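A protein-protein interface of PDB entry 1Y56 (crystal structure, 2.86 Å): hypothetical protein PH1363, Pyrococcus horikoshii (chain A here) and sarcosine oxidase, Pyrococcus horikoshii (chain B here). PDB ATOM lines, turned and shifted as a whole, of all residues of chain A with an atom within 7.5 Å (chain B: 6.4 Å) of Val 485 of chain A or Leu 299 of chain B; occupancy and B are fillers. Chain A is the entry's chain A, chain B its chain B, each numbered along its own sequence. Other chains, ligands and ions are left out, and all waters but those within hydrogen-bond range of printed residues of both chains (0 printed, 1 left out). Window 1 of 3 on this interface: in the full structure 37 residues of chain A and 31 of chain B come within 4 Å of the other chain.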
ATOM      1  N   PRO A  61      35.701  20.647   2.277  1.00  0.00           N
ATOM      2  CA  PRO A  61      34.650  21.656   2.108  1.00  0.00           C
ATOM      3  C   PRO A  61      35.060  22.828   1.194  1.00  0.00           C
ATOM      4  O   PRO A  61      36.256  23.076   0.966  1.00  0.00           O
ATOM      5  CB  PRO A  61      34.412  22.145   3.538  1.00  0.00           C
ATOM      6  CG  PRO A  61      35.767  22.009   4.209  1.00  0.00           C
ATOM      7  CD  PRO A  61      36.474  20.852   3.520  1.00  0.00           C
ATOM      8  N   GLY A  71      32.024  32.329   4.127  1.00  0.00           N
ATOM      9  CA  GLY A  71      31.917  30.985   4.663  1.00  0.00           C
ATOM     10  C   GLY A  71      30.692  30.155   4.332  1.00  0.00           C
ATOM     11  O   GLY A  71      30.408  29.196   5.042  1.00  0.00           O
ATOM     12  N   GLU A  73      28.774  27.337   1.995  1.00  0.00           N
ATOM     13  CA  GLU A  73      29.299  26.164   1.293  1.00  0.00           C
ATOM     14  C   GLU A  73      28.841  26.119  -0.153  1.00  0.00           C
ATOM     15  O   GLU A  73      27.644  26.013  -0.438  1.00  0.00           O
ATOM     16  CB  GLU A  73      28.935  24.859   2.006  1.00  0.00           C
ATOM     17  CG  GLU A  73      30.148  23.939   2.274  1.00  0.00           C
ATOM     18  CD  GLU A  73      30.681  23.183   1.044  1.00  0.00           C
ATOM     19  OE1 GLU A  73      30.042  23.181  -0.036  1.00  0.00           O
ATOM     20  OE2 GLU A  73      31.760  22.569   1.178  1.00  0.00           O
ATOM     21  N   ARG A  76      26.298  23.639  -1.678  1.00  0.00           N
ATOM     22  CA  ARG A  76      24.938  23.771  -1.192  1.00  0.00           C
ATOM     23  C   ARG A  76      24.210  24.962  -1.812  1.00  0.00           C
ATOM     24  O   ARG A  76      22.986  25.040  -1.719  1.00  0.00           O
ATOM     25  CB  ARG A  76      24.911  23.811   0.345  1.00  0.00           C
ATOM     26  CG  ARG A  76      24.728  22.423   0.996  1.00  0.00           C
ATOM     27  CD  ARG A  76      25.750  22.145   2.119  1.00  0.00           C
ATOM     28  NE  ARG A  76      25.625  23.060   3.267  1.00  0.00           N
ATOM     29  CZ  ARG A  76      26.548  23.240   4.228  1.00  0.00           C
ATOM     30  NH1 ARG A  76      27.703  22.571   4.210  1.00  0.00           N
ATOM     31  NH2 ARG A  76      26.320  24.102   5.220  1.00  0.00           N
ATOM     32  N   SER A 182      19.190  16.375   5.521  1.00  0.00           N
ATOM     33  CA  SER A 182      20.252  15.683   6.250  1.00  0.00           C
ATOM     34  C   SER A 182      19.792  15.128   7.590  1.00  0.00           C
ATOM     35  O   SER A 182      19.383  15.887   8.468  1.00  0.00           O
ATOM     36  CB  SER A 182      21.438  16.629   6.483  1.00  0.00           C
ATOM     37  OG  SER A 182      22.196  16.794   5.295  1.00  0.00           O
ATOM     38  N   LEU A 184      20.629  13.705  11.178  1.00  0.00           N
ATOM     39  CA  LEU A 184      21.726  13.990  12.090  1.00  0.00           C
ATOM     40  C   LEU A 184      22.130  12.781  12.942  1.00  0.00           C
ATOM     41  O   LEU A 184      23.111  12.826  13.683  1.00  0.00           O
ATOM     42  CB  LEU A 184      21.379  15.190  12.968  1.00  0.00           C
ATOM     43  CG  LEU A 184      21.050  16.483  12.218  1.00  0.00           C
ATOM     44  CD1 LEU A 184      20.677  17.588  13.194  1.00  0.00           C
ATOM     45  CD2 LEU A 184      22.212  16.897  11.321  1.00  0.00           C
ATOM     46  N   VAL A 197      16.275  15.748  11.700  1.00  0.00           N
ATOM     47  CA  VAL A 197      16.552  15.929  10.296  1.00  0.00           C
ATOM     48  C   VAL A 197      16.610  17.425   9.999  1.00  0.00           C
ATOM     49  O   VAL A 197      15.858  18.202  10.591  1.00  0.00           O
ATOM     50  CB  VAL A 197      15.461  15.170   9.484  1.00  0.00           C
ATOM     51  CG1 VAL A 197      14.705  16.065   8.489  1.00  0.00           C
ATOM     52  CG2 VAL A 197      16.043  13.944   8.828  1.00  0.00           C
ATOM     53  N   VAL A 198      17.522  17.834   9.117  1.00  0.00           N
ATOM     54  CA  VAL A 198      17.622  19.251   8.719  1.00  0.00           C
ATOM     55  C   VAL A 198      17.313  19.454   7.237  1.00  0.00           C
ATOM     56  O   VAL A 198      17.939  18.837   6.378  1.00  0.00           O
ATOM     57  CB  VAL A 198      19.014  19.855   9.016  1.00  0.00           C
ATOM     58  CG1 VAL A 198      19.035  21.349   8.679  1.00  0.00           C
ATOM     59  CG2 VAL A 198      19.405  19.629  10.450  1.00  0.00           C
ATOM     60  N   ASP A 201      16.804  25.259   6.383  1.00  0.00           N
ATOM     61  CA  ASP A 201      17.361  25.541   7.702  1.00  0.00           C
ATOM     62  C   ASP A 201      16.380  25.239   8.853  1.00  0.00           C
ATOM     63  O   ASP A 201      16.640  25.599   9.999  1.00  0.00           O
ATOM     64  CB  ASP A 201      17.899  26.981   7.770  1.00  0.00           C
ATOM     65  CG  ASP A 201      16.784  28.040   7.721  1.00  0.00           C
ATOM     66  OD1 ASP A 201      17.060  29.186   7.266  1.00  0.00           O
ATOM     67  OD2 ASP A 201      15.637  27.738   8.142  1.00  0.00           O
ATOM     68  N   LEU A 203      14.728  22.633  11.419  1.00  0.00           N
ATOM     69  CA  LEU A 203      14.962  21.330  12.013  1.00  0.00           C
ATOM     70  C   LEU A 203      13.636  20.580  12.047  1.00  0.00           C
ATOM     71  O   LEU A 203      12.629  21.157  12.428  1.00  0.00           O
ATOM     72  CB  LEU A 203      15.504  21.488  13.426  1.00  0.00           C
ATOM     73  CG  LEU A 203      15.619  20.225  14.275  1.00  0.00           C
ATOM     74  CD1 LEU A 203      16.684  19.285  13.717  1.00  0.00           C
ATOM     75  CD2 LEU A 203      15.916  20.588  15.725  1.00  0.00           C
ATOM     76  N   PHE A 448      35.770  18.074   8.166  1.00  0.00           N
ATOM     77  CA  PHE A 448      34.333  18.236   8.069  1.00  0.00           C
ATOM     78  C   PHE A 448      33.676  16.995   7.422  1.00  0.00           C
ATOM     79  O   PHE A 448      32.447  16.818   7.615  1.00  0.00           O
ATOM     80  CB  PHE A 448      34.068  19.235   6.912  1.00  0.00           C
ATOM     81  CG  PHE A 448      34.190  20.690   7.264  1.00  0.00           C
ATOM     82  CD1 PHE A 448      35.357  21.211   7.857  1.00  0.00           C
ATOM     83  CD2 PHE A 448      33.144  21.570   6.925  1.00  0.00           C
ATOM     84  CE1 PHE A 448      35.461  22.593   8.172  1.00  0.00           C
ATOM     85  CE2 PHE A 448      33.233  22.940   7.225  1.00  0.00           C
ATOM     86  CZ  PHE A 448      34.403  23.455   7.861  1.00  0.00           C
ATOM     87  N   PRO A 481      26.371  14.376  15.777  1.00  0.00           N
ATOM     88  CA  PRO A 481      25.712  14.702  14.504  1.00  0.00           C
ATOM     89  C   PRO A 481      26.506  14.038  13.394  1.00  0.00           C
ATOM     90  O   PRO A 481      27.655  14.399  13.177  1.00  0.00           O
ATOM     91  CB  PRO A 481      25.787  16.232  14.432  1.00  0.00           C
ATOM     92  CG  PRO A 481      26.922  16.625  15.333  1.00  0.00           C
ATOM     93  CD  PRO A 481      27.337  15.418  16.178  1.00  0.00           C
ATOM     94  N   ILE A 482      25.930  13.039  12.733  1.00  0.00           N
ATOM     95  CA  ILE A 482      26.668  12.319  11.693  1.00  0.00           C
ATOM     96  C   ILE A 482      26.909  13.204  10.464  1.00  0.00           C
ATOM     97  O   ILE A 482      27.834  12.961   9.681  1.00  0.00           O
ATOM     98  CB  ILE A 482      26.034  10.952  11.311  1.00  0.00           C
ATOM     99  CG1 ILE A 482      24.606  11.110  10.777  1.00  0.00           C
ATOM    100  CG2 ILE A 482      26.090  10.000  12.485  1.00  0.00           C
ATOM    101  CD1 ILE A 482      24.124   9.912   9.985  1.00  0.00           C
ATOM    102  N   LYS A 483      26.085  14.237  10.323  1.00  0.00           N
ATOM    103  CA  LYS A 483      26.282  15.247   9.305  1.00  0.00           C
ATOM    104  C   LYS A 483      26.408  16.617   9.945  1.00  0.00           C
ATOM    105  O   LYS A 483      25.761  16.888  10.957  1.00  0.00           O
ATOM    106  CB  LYS A 483      25.123  15.240   8.316  1.00  0.00           C
ATOM    107  CG  LYS A 483      25.112  14.042   7.401  1.00  0.00           C
ATOM    108  CD  LYS A 483      26.162  14.145   6.310  1.00  0.00           C
ATOM    109  CE  LYS A 483      25.949  13.022   5.312  1.00  0.00           C
ATOM    110  NZ  LYS A 483      27.145  12.714   4.478  1.00  0.00           N
ATOM    111  N   ASN A 484      27.251  17.466   9.351  1.00  0.00           N
ATOM    112  CA  ASN A 484      27.435  18.847   9.791  1.00  0.00           C
ATOM    113  C   ASN A 484      26.118  19.588   9.831  1.00  0.00           C
ATOM    114  O   ASN A 484      25.361  19.588   8.862  1.00  0.00           O
ATOM    115  CB  ASN A 484      28.363  19.615   8.841  1.00  0.00           C
ATOM    116  CG  ASN A 484      29.792  19.114   8.862  1.00  0.00           C
ATOM    117  OD1 ASN A 484      30.162  18.274   9.694  1.00  0.00           O
ATOM    118  ND2 ASN A 484      30.613  19.631   7.933  1.00  0.00           N
ATOM    119  N   VAL A 485      25.859  20.225  10.960  1.00  0.00           N
ATOM    120  CA  VAL A 485      24.718  21.107  11.122  1.00  0.00           C
ATOM    121  C   VAL A 485      25.199  22.349  11.873  1.00  0.00           C
ATOM    122  O   VAL A 485      26.078  22.279  12.737  1.00  0.00           O
ATOM    123  CB  VAL A 485      23.560  20.397  11.865  1.00  0.00           C
ATOM    124  CG1 VAL A 485      24.023  19.824  13.220  1.00  0.00           C
ATOM    125  CG2 VAL A 485      22.380  21.329  12.036  1.00  0.00           C
ATOM    126  N   LYS A 486      24.646  23.494  11.528  1.00  0.00           N
ATOM    127  CA  LYS A 486      25.048  24.727  12.180  1.00  0.00           C
ATOM    128  C   LYS A 486      23.829  25.351  12.758  1.00  0.00           C
ATOM    129  O   LYS A 486      22.759  25.139  12.219  1.00  0.00           O
ATOM    130  CB  LYS A 486      25.561  25.725  11.129  1.00  0.00           C
ATOM    131  CG  LYS A 486      24.671  25.850   9.873  1.00  0.00           C
ATOM    132  CD  LYS A 486      24.495  27.297   9.415  1.00  0.00           C
ATOM    133  CE  LYS A 486      25.687  27.824   8.615  1.00  0.00           C
ATOM    134  NZ  LYS A 486      25.575  27.557   7.155  1.00  0.00           N
ATOM    135  N   MET A 487      23.903  26.033  13.890  1.00  0.00           N
ATOM    136  CA  MET A 487      24.216  25.530  15.201  1.00  0.00           C
ATOM    137  C   MET A 487      23.021  26.334  15.677  1.00  0.00           C
ATOM    138  O   MET A 487      22.266  25.928  16.565  1.00  0.00           O
ATOM    139  CB  MET A 487      25.478  26.098  15.862  1.00  0.00           C
ATOM    140  CG  MET A 487      25.333  26.028  17.412  1.00  0.00           C
ATOM    141  SD  MET A 487      26.627  26.474  18.606  1.00  0.00           S
ATOM    142  CE  MET A 487      27.526  24.943  18.793  1.00  0.00           C
ATOM    143  N   GLY A 488      22.857  27.489  15.025  1.00  0.00           N
ATOM    144  CA  GLY A 488      21.644  28.285  15.086  1.00  0.00           C
ATOM    145  C   GLY A 488      20.404  27.446  14.825  1.00  0.00           C
ATOM    146  O   GLY A 488      19.413  27.567  15.546  1.00  0.00           O
ATOM    147  N   ILE A 489      20.476  26.575  13.817  1.00  0.00           N
ATOM    148  CA  ILE A 489      19.386  25.658  13.470  1.00  0.00           C
ATOM    149  C   ILE A 489      18.957  24.803  14.664  1.00  0.00           C
ATOM    150  O   ILE A 489      17.826  24.358  14.720  1.00  0.00           O
ATOM    151  CB  ILE A 489      19.760  24.761  12.249  1.00  0.00           C
ATOM    152  CG1 ILE A 489      19.772  25.585  10.957  1.00  0.00           C
ATOM    153  CG2 ILE A 489      18.804  23.584  12.099  1.00  0.00           C
ATOM    154  CD1 ILE A 489      20.514  24.934   9.810  1.00  0.00           C
ATOM    155  N   LEU A 490      19.844  24.604  15.629  1.00  0.00           N
ATOM    156  CA  LEU A 490      19.536  23.763  16.775  1.00  0.00           C
ATOM    157  C   LEU A 490      19.101  24.487  18.067  1.00  0.00           C
ATOM    158  O   LEU A 490      19.023  23.851  19.115  1.00  0.00           O
ATOM    159  CB  LEU A 490      20.721  22.850  17.056  1.00  0.00           C
ATOM    160  CG  LEU A 490      20.876  21.451  16.461  1.00  0.00           C
ATOM    161  CD1 LEU A 490      20.227  21.298  15.123  1.00  0.00           C
ATOM    162  CD2 LEU A 490      22.342  21.140  16.367  1.00  0.00           C
ATOM    163  N   ILE B 229      32.412  20.399  19.471  1.00  0.00           N
ATOM    164  CA  ILE B 229      33.459  21.117  18.754  1.00  0.00           C
ATOM    165  C   ILE B 229      32.859  21.674  17.465  1.00  0.00           C
ATOM    166  O   ILE B 229      32.110  20.982  16.767  1.00  0.00           O
ATOM    167  CB  ILE B 229      34.710  20.218  18.466  1.00  0.00           C
ATOM    168  CG1 ILE B 229      35.840  21.030  17.846  1.00  0.00           C
ATOM    169  CG2 ILE B 229      34.360  19.015  17.554  1.00  0.00           C
ATOM    170  CD1 ILE B 229      36.405  22.034  18.766  1.00  0.00           C
ATOM    171  N   THR B 230      33.163  22.929  17.157  1.00  0.00           N
ATOM    172  CA  THR B 230      32.701  23.506  15.903  1.00  0.00           C
ATOM    173  C   THR B 230      33.799  23.421  14.850  1.00  0.00           C
ATOM    174  O   THR B 230      34.894  22.921  15.115  1.00  0.00           O
ATOM    175  CB  THR B 230      32.259  24.963  16.066  1.00  0.00           C
ATOM    176  OG1 THR B 230      33.387  25.827  15.902  1.00  0.00           O
ATOM    177  CG2 THR B 230      31.652  25.199  17.428  1.00  0.00           C
ATOM    178  N   GLN B 231      33.492  23.902  13.649  1.00  0.00           N
ATOM    179  CA  GLN B 231      34.476  24.020  12.580  1.00  0.00           C
ATOM    180  C   GLN B 231      35.513  25.066  12.975  1.00  0.00           C
ATOM    181  O   GLN B 231      35.203  25.959  13.752  1.00  0.00           O
ATOM    182  CB  GLN B 231      33.789  24.436  11.299  1.00  0.00           C
ATOM    183  CG  GLN B 231      33.134  25.778  11.390  1.00  0.00           C
ATOM    184  CD  GLN B 231      32.631  26.249  10.053  1.00  0.00           C
ATOM    185  OE1 GLN B 231      31.416  26.295   9.803  1.00  0.00           O
ATOM    186  NE2 GLN B 231      33.563  26.593   9.168  1.00  0.00           N
ATOM    187  N   LEU B 281      22.916  18.168  22.451  1.00  0.00           N
ATOM    188  CA  LEU B 281      23.129  18.841  21.167  1.00  0.00           C
ATOM    189  C   LEU B 281      22.267  20.098  21.074  1.00  0.00           C
ATOM    190  O   LEU B 281      22.731  21.163  20.667  1.00  0.00           O
ATOM    191  CB  LEU B 281      22.769  17.910  20.009  1.00  0.00           C
ATOM    192  CG  LEU B 281      23.573  17.844  18.695  1.00  0.00           C
ATOM    193  CD1 LEU B 281      22.615  17.691  17.519  1.00  0.00           C
ATOM    194  CD2 LEU B 281      24.501  19.038  18.470  1.00  0.00           C
ATOM    195  N   LEU B 295      28.182  32.291  16.638  1.00  0.00           N
ATOM    196  CA  LEU B 295      28.128  30.822  16.668  1.00  0.00           C
ATOM    197  C   LEU B 295      26.950  30.213  15.895  1.00  0.00           C
ATOM    198  O   LEU B 295      27.048  29.088  15.417  1.00  0.00           O
ATOM    199  CB  LEU B 295      28.148  30.309  18.112  1.00  0.00           C
ATOM    200  CG  LEU B 295      29.468  29.950  18.826  1.00  0.00           C
ATOM    201  CD1 LEU B 295      30.716  30.666  18.314  1.00  0.00           C
ATOM    202  CD2 LEU B 295      29.343  30.140  20.339  1.00  0.00           C
ATOM    203  N   LYS B 296      25.853  30.956  15.753  1.00  0.00           N
ATOM    204  CA  LYS B 296      24.721  30.520  14.917  1.00  0.00           C
ATOM    205  C   LYS B 296      25.090  30.094  13.487  1.00  0.00           C
ATOM    206  O   LYS B 296      24.516  29.143  12.957  1.00  0.00           O
ATOM    207  CB  LYS B 296      23.643  31.600  14.857  1.00  0.00           C
ATOM    208  CG  LYS B 296      22.877  31.747  16.136  1.00  0.00           C
ATOM    209  CD  LYS B 296      21.751  32.703  15.982  1.00  0.00           C
ATOM    210  CE  LYS B 296      21.140  32.983  17.330  1.00  0.00           C
ATOM    211  NZ  LYS B 296      19.957  33.884  17.208  1.00  0.00           N
ATOM    212  N   ASN B 297      26.042  30.795  12.871  1.00  0.00           N
ATOM    213  CA  ASN B 297      26.455  30.501  11.490  1.00  0.00           C
ATOM    214  C   ASN B 297      27.519  29.395  11.397  1.00  0.00           C
ATOM    215  O   ASN B 297      27.952  29.021  10.304  1.00  0.00           O
ATOM    216  CB  ASN B 297      26.964  31.767  10.777  1.00  0.00           C
ATOM    217  CG  ASN B 297      26.138  33.021  11.100  1.00  0.00           C
ATOM    218  OD1 ASN B 297      24.915  32.964  11.316  1.00  0.00           O
ATOM    219  ND2 ASN B 297      26.817  34.169  11.130  1.00  0.00           N
ATOM    220  N   LEU B 298      27.924  28.868  12.545  1.00  0.00           N
ATOM    221  CA  LEU B 298      28.985  27.871  12.590  1.00  0.00           C
ATOM    222  C   LEU B 298      28.517  26.412  12.612  1.00  0.00           C
ATOM    223  O   LEU B 298      27.645  26.029  13.400  1.00  0.00           O
ATOM    224  CB  LEU B 298      29.902  28.153  13.778  1.00  0.00           C
ATOM    225  CG  LEU B 298      31.151  29.003  13.536  1.00  0.00           C
ATOM    226  CD1 LEU B 298      31.051  29.893  12.303  1.00  0.00           C
ATOM    227  CD2 LEU B 298      31.430  29.812  14.777  1.00  0.00           C
ATOM    228  N   LEU B 299      29.118  25.611  11.734  1.00  0.00           N
ATOM    229  CA  LEU B 299      28.899  24.172  11.686  1.00  0.00           C
ATOM    230  C   LEU B 299      29.378  23.456  12.959  1.00  0.00           C
ATOM    231  O   LEU B 299      30.510  23.685  13.418  1.00  0.00           O
ATOM    232  CB  LEU B 299      29.656  23.608  10.491  1.00  0.00           C
ATOM    233  CG  LEU B 299      28.995  23.299   9.147  1.00  0.00           C
ATOM    234  CD1 LEU B 299      27.560  23.766   9.044  1.00  0.00           C
ATOM    235  CD2 LEU B 299      29.841  23.872   8.030  1.00  0.00           C
ATOM    236  N   ILE B 300      28.518  22.605  13.528  1.00  0.00           N
ATOM    237  CA  ILE B 300      28.952  21.648  14.553  1.00  0.00           C
ATOM    238  C   ILE B 300      29.501  20.423  13.841  1.00  0.00           C
ATOM    239  O   ILE B 300      28.861  19.921  12.927  1.00  0.00           O
ATOM    240  CB  ILE B 300      27.804  21.208  15.461  1.00  0.00           C
ATOM    241  CG1 ILE B 300      27.351  22.359  16.339  1.00  0.00           C
ATOM    242  CG2 ILE B 300      28.238  20.057  16.346  1.00  0.00           C
ATOM    243  CD1 ILE B 300      25.968  22.170  16.910  1.00  0.00           C
ATOM    244  N   LEU B 301      30.677  19.950  14.251  1.00  0.00           N
ATOM    245  CA  LEU B 301      31.321  18.815  13.581  1.00  0.00           C
ATOM    246  C   LEU B 301      31.099  17.489  14.280  1.00  0.00           C
ATOM    247  O   LEU B 301      30.771  16.499  13.636  1.00  0.00           O
ATOM    248  CB  LEU B 301      32.824  19.046  13.422  1.00  0.00           C
ATOM    249  CG  LEU B 301      33.241  20.147  12.448  1.00  0.00           C
ATOM    250  CD1 LEU B 301      34.754  20.202  12.344  1.00  0.00           C
ATOM    251  CD2 LEU B 301      32.605  19.965  11.075  1.00  0.00           C
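O of Lys 296 of chain B lies within hydrogen-bond range of N of Met 487 of chain A.
N of Ile 300 of chain B is in hydrogen-bond range of O of Val 485 of chain A (2.6 Å).
N of Gly 488 of chain A sits at hydrogen-bond distance from O of Lys 296 of chain B (3.1 Å).
The side-chain amide nitrogen (ND2) of Asn 484 of chain A sits close to the backbone carbonyl oxygen (O) of Phe 448 of chain A, 3.4 Å away.
The backbone carbonyl oxygen (O) of Leu 299 of chain B is in hydrogen-bond range of the backbone NH (N) of Gln 231 of chain B (3.0 Å).
The backbone carbonyl oxygen of Ile 229 of chain B is in hydrogen-bond range of the backbone NH of Leu 301 of chain B (3.1 Å).
Among the printed residues, pairs that only touch across the chains: Phe 448 of chain A with Gln 231 of chain B (3.5 Å), Phe 448 of chain A with Leu 299 of chain B (3.6 Å), Phe 448 of chain A with Leu 301 of chain B (3.9 Å), Pro 481 of chain A with Ile 300 of chain B (3.8 Å), Pro 481 of chain A with Leu 301 of chain B (3.8 Å), Asn 484 of chain A with Leu 299 of chain B (3.8 Å), Asn 484 of chain A with Ile 300 of chain B (3.6 Å), Asn 484 of chain A with Leu 301 of chain B (3.3 Å), Val 485 of chain A with Leu 299 of chain B (3.5 Å), Lys 486 of chain A with Lys 296 of chain B (3.9 Å), Lys 486 of chain A with Asn 297 of chain B (3.1 Å), Lys 486 of chain A with Leu 298 of chain B (3.1 Å), Lys 486 of chain A with Leu 299 of chain B (3.5 Å), Met 487 of chain A with Leu 295 of chain B (3.4 Å), Met 487 of chain A with Leu 298 of chain B (3.3 Å), Met 487 of chain A with Ile 300 of chain B (3.6 Å), Leu 490 of chain A with Leu 281 of chain B (3.6 Å) and Leu 490 of chain A with Ile 300 of chain B (3.8 Å).
Val 485 of chain A touches just these residues of chain B: Leu 299 (3.5 Å) and Ile 300 (2.6 Å).
Of chain A, only Phe 448 (3.6 Å), Asn 484 (3.8 Å), Val 485 (3.5 Å) and Lys 486 (3.5 Å) come within 4 Å of Leu 299 of chain B.
Printed residues of chain A within 4 Å of Gln 231 of chain B: Phe 448 (3.5 Å).
Of the printed residues of chain A, Leu 298 of chain B touches Lys 486 (3.1 Å) and Met 487 (3.3 Å).
Of the printed residues of chain A, Leu 281 of chain B touches Leu 490 (3.6 Å).
Glu 73 of chain A touches none of the printed residues of chain B.
The nearest residue of chain A that does not touch Leu 299 of chain B is Arg 76 of chain A (4.03 Å).
Of the 21 printed residues of chain A, 8 touch a printed residue of chain B.
Hydrophobic or aromatic side chains of chain A that line the printed part of chain B: Phe 448, Pro 481, Met 487 and Leu 490.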
